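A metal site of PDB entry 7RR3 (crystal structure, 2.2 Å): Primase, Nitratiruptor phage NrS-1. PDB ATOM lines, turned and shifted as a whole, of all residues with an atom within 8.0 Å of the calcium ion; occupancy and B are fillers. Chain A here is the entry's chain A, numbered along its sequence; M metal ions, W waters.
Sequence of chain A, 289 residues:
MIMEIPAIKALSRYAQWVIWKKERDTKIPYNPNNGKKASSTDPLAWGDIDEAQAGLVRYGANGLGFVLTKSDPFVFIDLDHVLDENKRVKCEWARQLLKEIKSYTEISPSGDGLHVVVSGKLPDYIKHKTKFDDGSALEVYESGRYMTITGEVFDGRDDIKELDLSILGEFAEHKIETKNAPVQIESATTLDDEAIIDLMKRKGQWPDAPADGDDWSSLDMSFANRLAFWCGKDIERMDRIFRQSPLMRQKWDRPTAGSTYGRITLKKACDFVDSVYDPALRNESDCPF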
ATOM      1  N   GLN A  16       7.611  -0.003  19.391  1.00  0.00           N
ATOM      2  CA  GLN A  16       6.966   1.179  18.819  1.00  0.00           C
ATOM      3  C   GLN A  16       7.481   1.456  17.415  1.00  0.00           C
ATOM      4  O   GLN A  16       7.630   2.602  17.004  1.00  0.00           O
ATOM      5  CB  GLN A  16       7.188   2.394  19.721  1.00  0.00           C
ATOM      6  CG  GLN A  16       6.792   2.169  21.168  1.00  0.00           C
ATOM      7  CD  GLN A  16       7.168   3.338  22.059  1.00  0.00           C
ATOM      8  OE1 GLN A  16       7.633   4.377  21.579  1.00  0.00           O
ATOM      9  NE2 GLN A  16       6.979   3.181  23.360  1.00  0.00           N
ATOM     10  N   PHE A  66       9.745   5.100  13.946  1.00  0.00           N
ATOM     11  CA  PHE A  66       9.641   4.958  15.400  1.00  0.00           C
ATOM     12  C   PHE A  66       8.608   5.945  15.918  1.00  0.00           C
ATOM     13  O   PHE A  66       8.735   7.152  15.672  1.00  0.00           O
ATOM     14  CB  PHE A  66      10.995   5.179  16.075  1.00  0.00           C
ATOM     15  CG  PHE A  66      10.980   4.917  17.555  1.00  0.00           C
ATOM     16  CD1 PHE A  66      11.204   3.631  18.040  1.00  0.00           C
ATOM     17  CD2 PHE A  66      10.753   5.938  18.464  1.00  0.00           C
ATOM     18  CE1 PHE A  66      11.192   3.388  19.406  1.00  0.00           C
ATOM     19  CE2 PHE A  66      10.742   5.691  19.817  1.00  0.00           C
ATOM     20  CZ  PHE A  66      10.965   4.415  20.292  1.00  0.00           C
ATOM     21  N   VAL A  67       7.606   5.437  16.629  1.00  0.00           N
ATOM     22  CA  VAL A  67       6.501   6.258  17.112  1.00  0.00           C
ATOM     23  C   VAL A  67       6.885   6.861  18.452  1.00  0.00           C
ATOM     24  O   VAL A  67       7.277   6.152  19.383  1.00  0.00           O
ATOM     25  CB  VAL A  67       5.213   5.428  17.227  1.00  0.00           C
ATOM     26  CG1 VAL A  67       4.039   6.319  17.610  1.00  0.00           C
ATOM     27  CG2 VAL A  67       4.931   4.703  15.930  1.00  0.00           C
ATOM     28  N   LEU A  68       6.764   8.182  18.554  1.00  0.00           N
ATOM     29  CA  LEU A  68       7.013   8.901  19.800  1.00  0.00           C
ATOM     30  C   LEU A  68       5.753   8.900  20.650  1.00  0.00           C
ATOM     31  O   LEU A  68       4.679   9.292  20.177  1.00  0.00           O
ATOM     32  CB  LEU A  68       7.460  10.336  19.511  1.00  0.00           C
ATOM     33  CG  LEU A  68       8.502  10.529  18.414  1.00  0.00           C
ATOM     34  CD1 LEU A  68       8.526  11.984  17.971  1.00  0.00           C
ATOM     35  CD2 LEU A  68       9.866  10.080  18.885  1.00  0.00           C
ATOM     36  N   THR A  69       5.890   8.461  21.896  1.00  0.00           N
ATOM     37  CA  THR A  69       4.767   8.373  22.818  1.00  0.00           C
ATOM     38  C   THR A  69       5.016   9.266  24.028  1.00  0.00           C
ATOM     39  O   THR A  69       6.143   9.674  24.311  1.00  0.00           O
ATOM     40  CB  THR A  69       4.544   6.922  23.288  1.00  0.00           C
ATOM     41  OG1 THR A  69       5.558   6.564  24.232  1.00  0.00           O
ATOM     42  CG2 THR A  69       4.591   5.965  22.107  1.00  0.00           C
ATOM     43  N   LYS A  70       3.933   9.550  24.763  1.00  0.00           N
ATOM     44  CA  LYS A  70       4.023  10.342  25.977  1.00  0.00           C
ATOM     45  C   LYS A  70       4.750   9.623  27.108  1.00  0.00           C
ATOM     46  O   LYS A  70       4.937  10.219  28.178  1.00  0.00           O
ATOM     47  CB  LYS A  70       2.629  10.746  26.450  1.00  0.00           C
ATOM     48  CG  LYS A  70       1.874  11.634  25.495  1.00  0.00           C
ATOM     49  CD  LYS A  70       0.541  12.058  26.089  1.00  0.00           C
ATOM     50  CE  LYS A  70      -0.406  12.547  25.014  1.00  0.00           C
ATOM     51  NZ  LYS A  70      -0.261  14.003  24.794  1.00  0.00           N
ATOM     52  N   SER A  71       5.151   8.377  26.905  1.00  0.00           N
ATOM     53  CA  SER A  71       5.796   7.588  27.947  1.00  0.00           C
ATOM     54  C   SER A  71       7.271   7.332  27.704  1.00  0.00           C
ATOM     55  O   SER A  71       7.973   6.912  28.634  1.00  0.00           O
ATOM     56  CB  SER A  71       5.072   6.241  28.107  1.00  0.00           C
ATOM     57  OG  SER A  71       3.694   6.435  28.392  1.00  0.00           O
ATOM     58  N   ASP A  72       7.775   7.566  26.492  1.00  0.00           N
ATOM     59  CA  ASP A  72       9.200   7.476  26.212  1.00  0.00           C
ATOM     60  C   ASP A  72       9.794   8.867  26.007  1.00  0.00           C
ATOM     61  O   ASP A  72       9.099   9.776  25.530  1.00  0.00           O
ATOM     62  CB  ASP A  72       9.468   6.600  24.977  1.00  0.00           C
ATOM     63  CG  ASP A  72       9.004   7.251  23.685  1.00  0.00           C
ATOM     64  OD1 ASP A  72       7.829   7.041  23.306  1.00  0.00           O
ATOM     65  OD2 ASP A  72       9.804   7.961  23.060  1.00  0.00           O
ATOM     66  N   PRO A  73      11.058   9.074  26.367  1.00  0.00           N
ATOM     67  CA  PRO A  73      11.585  10.442  26.464  1.00  0.00           C
ATOM     68  C   PRO A  73      12.326  10.952  25.230  1.00  0.00           C
ATOM     69  O   PRO A  73      13.061  11.938  25.322  1.00  0.00           O
ATOM     70  CB  PRO A  73      12.541  10.331  27.657  1.00  0.00           C
ATOM     71  CG  PRO A  73      13.132   8.959  27.479  1.00  0.00           C
ATOM     72  CD  PRO A  73      12.040   8.093  26.867  1.00  0.00           C
ATOM     73  N   PHE A  74      12.129  10.309  24.084  1.00  0.00           N
ATOM     74  CA  PHE A  74      12.885  10.683  22.893  1.00  0.00           C
ATOM     75  C   PHE A  74      12.279  11.915  22.222  1.00  0.00           C
ATOM     76  O   PHE A  74      11.061  11.965  21.982  1.00  0.00           O
ATOM     77  CB  PHE A  74      12.944   9.504  21.921  1.00  0.00           C
ATOM     78  CG  PHE A  74      13.596   8.285  22.495  1.00  0.00           C
ATOM     79  CD1 PHE A  74      14.951   8.290  22.779  1.00  0.00           C
ATOM     80  CD2 PHE A  74      12.860   7.152  22.761  1.00  0.00           C
ATOM     81  CE1 PHE A  74      15.564   7.163  23.321  1.00  0.00           C
ATOM     82  CE2 PHE A  74      13.461   6.031  23.301  1.00  0.00           C
ATOM     83  CZ  PHE A  74      14.816   6.036  23.585  1.00  0.00           C
ATOM     84  N   VAL A  75      13.121  12.896  21.926  1.00  0.00           N
ATOM     85  CA  VAL A  75      12.712  14.137  21.284  1.00  0.00           C
ATOM     86  C   VAL A  75      13.198  14.122  19.843  1.00  0.00           C
ATOM     87  O   VAL A  75      14.382  13.896  19.586  1.00  0.00           O
ATOM     88  CB  VAL A  75      13.254  15.363  22.044  1.00  0.00           C
ATOM     89  CG1 VAL A  75      12.785  16.652  21.380  1.00  0.00           C
ATOM     90  CG2 VAL A  75      12.830  15.316  23.504  1.00  0.00           C
ATOM     91  N   PHE A  76      12.283  14.377  18.922  1.00  0.00           N
ATOM     92  CA  PHE A  76      12.581  14.367  17.485  1.00  0.00           C
ATOM     93  C   PHE A  76      12.766  15.804  17.017  1.00  0.00           C
ATOM     94  O   PHE A  76      11.811  16.570  16.944  1.00  0.00           O
ATOM     95  CB  PHE A  76      11.457  13.666  16.722  1.00  0.00           C
ATOM     96  CG  PHE A  76      11.570  13.793  15.221  1.00  0.00           C
ATOM     97  CD1 PHE A  76      12.787  13.659  14.586  1.00  0.00           C
ATOM     98  CD2 PHE A  76      10.439  14.035  14.462  1.00  0.00           C
ATOM     99  CE1 PHE A  76      12.878  13.768  13.212  1.00  0.00           C
ATOM    100  CE2 PHE A  76      10.521  14.137  13.083  1.00  0.00           C
ATOM    101  CZ  PHE A  76      11.748  14.010  12.453  1.00  0.00           C
ATOM    102  N   VAL A 118      17.069  13.420  20.829  1.00  0.00           N
ATOM    103  CA  VAL A 118      17.552  13.774  22.155  1.00  0.00           C
ATOM    104  C   VAL A 118      16.611  13.171  23.184  1.00  0.00           C
ATOM    105  O   VAL A 118      15.402  13.096  22.968  1.00  0.00           O
ATOM    106  CB  VAL A 118      17.650  15.301  22.339  1.00  0.00           C
ATOM    107  CG1 VAL A 118      18.165  15.665  23.729  1.00  0.00           C
ATOM    108  CG2 VAL A 118      18.554  15.912  21.262  1.00  0.00           C
ATOM    109  N   GLY A 120      15.079  14.085  26.383  1.00  0.00           N
ATOM    110  CA  GLY A 120      14.856  15.231  27.247  1.00  0.00           C
ATOM    111  C   GLY A 120      13.427  15.747  27.230  1.00  0.00           C
ATOM    112  O   GLY A 120      12.483  14.974  27.054  1.00  0.00           O
ATOM    113  N   LYS A 121      13.274  17.057  27.407  1.00  0.00           N
ATOM    114  CA  LYS A 121      11.966  17.690  27.468  1.00  0.00           C
ATOM    115  C   LYS A 121      12.024  19.010  26.710  1.00  0.00           C
ATOM    116  O   LYS A 121      12.935  19.810  26.929  1.00  0.00           O
ATOM    117  CB  LYS A 121      11.539  17.919  28.925  1.00  0.00           C
ATOM    118  CG  LYS A 121      10.293  18.782  29.078  1.00  0.00           C
ATOM    119  CD  LYS A 121       9.052  18.039  28.626  1.00  0.00           C
ATOM    120  CE  LYS A 121       7.950  19.001  28.228  1.00  0.00           C
ATOM    121  NZ  LYS A 121       6.850  18.298  27.509  1.00  0.00           N
ATOM    122  N   TYR A 141       9.206  17.577  18.060  1.00  0.00           N
ATOM    123  CA  TYR A 141       8.085  16.728  18.413  1.00  0.00           C
ATOM    124  C   TYR A 141       8.470  15.809  19.557  1.00  0.00           C
ATOM    125  O   TYR A 141       9.602  15.315  19.614  1.00  0.00           O
ATOM    126  CB  TYR A 141       7.616  15.893  17.216  1.00  0.00           C
ATOM    127  CG  TYR A 141       7.140  16.725  16.038  1.00  0.00           C
ATOM    128  CD1 TYR A 141       5.943  17.431  16.116  1.00  0.00           C
ATOM    129  CD2 TYR A 141       7.879  16.805  14.876  1.00  0.00           C
ATOM    130  CE1 TYR A 141       5.502  18.192  15.053  1.00  0.00           C
ATOM    131  CE2 TYR A 141       7.451  17.556  13.801  1.00  0.00           C
ATOM    132  CZ  TYR A 141       6.262  18.251  13.896  1.00  0.00           C
ATOM    133  OH  TYR A 141       5.821  19.012  12.833  1.00  0.00           O
ATOM    134  N   GLU A 142       7.527  15.581  20.471  1.00  0.00           N
ATOM    135  CA  GLU A 142       7.735  14.745  21.637  1.00  0.00           C
ATOM    136  C   GLU A 142       6.840  13.516  21.680  1.00  0.00           C
ATOM    137  O   GLU A 142       7.255  12.490  22.224  1.00  0.00           O
ATOM    138  CB  GLU A 142       7.525  15.548  22.930  1.00  0.00           C
ATOM    139  CG  GLU A 142       8.797  16.132  23.511  1.00  0.00           C
ATOM    140  CD  GLU A 142       8.523  17.122  24.630  1.00  0.00           C
ATOM    141  OE1 GLU A 142       7.370  17.596  24.738  1.00  0.00           O
ATOM    142  OE2 GLU A 142       9.453  17.432  25.402  1.00  0.00           O
ATOM    143  N   SER A 143       5.630  13.595  21.133  1.00  0.00           N
ATOM    144  CA  SER A 143       4.694  12.474  21.161  1.00  0.00           C
ATOM    145  C   SER A 143       3.655  12.698  20.075  1.00  0.00           C
ATOM    146  O   SER A 143       3.705  13.670  19.330  1.00  0.00           O
ATOM    147  CB  SER A 143       4.048  12.317  22.544  1.00  0.00           C
ATOM    148  OG  SER A 143       3.310  13.478  22.878  1.00  0.00           O
ATOM    149  N   GLY A 144       2.694  11.773  20.002  1.00  0.00           N
ATOM    150  CA  GLY A 144       1.643  11.851  19.003  1.00  0.00           C
ATOM    151  C   GLY A 144       2.153  11.873  17.575  1.00  0.00           C
ATOM    152  O   GLY A 144       1.498  12.428  16.693  1.00  0.00           O
ATOM    153  N   ARG A 145       3.304  11.266  17.332  1.00  0.00           N
ATOM    154  CA  ARG A 145       3.951  11.339  16.036  1.00  0.00           C
ATOM    155  C   ARG A 145       4.979  10.229  15.921  1.00  0.00           C
ATOM    156  O   ARG A 145       5.445   9.683  16.924  1.00  0.00           O
ATOM    157  CB  ARG A 145       4.614  12.706  15.825  1.00  0.00           C
ATOM    158  CG  ARG A 145       4.755  13.128  14.376  1.00  0.00           C
ATOM    159  CD  ARG A 145       4.916  14.633  14.254  1.00  0.00           C
ATOM    160  NE  ARG A 145       3.640  15.321  14.428  1.00  0.00           N
ATOM    161  CZ  ARG A 145       3.173  16.240  13.601  1.00  0.00           C
ATOM    162  NH1 ARG A 145       3.847  16.613  12.523  1.00  0.00           N
ATOM    163  NH2 ARG A 145       1.994  16.795  13.856  1.00  0.00           N
HETATM  164 CA    CA M   1       7.953  11.358  24.238  1.00  0.00          CA
HETATM  165  O   HOH W   1       9.083  10.263  22.358  1.00  0.00           O
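The side-chain carboxylate (OD1) of Asp 72 sits at hydrogen-bond distance from the side-chain hydroxyl (OG1) of Thr 69. The backbone NH of Phe 74 lies close to the side-chain carboxylate of Asp 72 (3.5 Å). OE1 of Gln 16 sits close to OD1 of Asp 72. OE1 of Glu 142 lies within salt-bridge range of NZ of Lys 121, 2.9 Å away. The side-chain hydroxyl (OG1) of Thr 69 sits close to the backbone NH (N) of Ser 71 (3.3 Å).
Phe 74 touches the calcium ion. Within 4 Å of the calcium ion: Thr 69, Asp 72, Phe 74 and Glu 142. The nearest printed residue that does not touch the calcium ion is Pro 73 (4.4 Å).
The calcium ion is bound by O of Asp 72 (2.3 Å), O of Glu 142 (2.4 Å), water W1 (2.5 Å) and O of Thr 69 (2.5 Å).
Water W1 bridges OD2 of Asp 72 and O of Phe 74.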
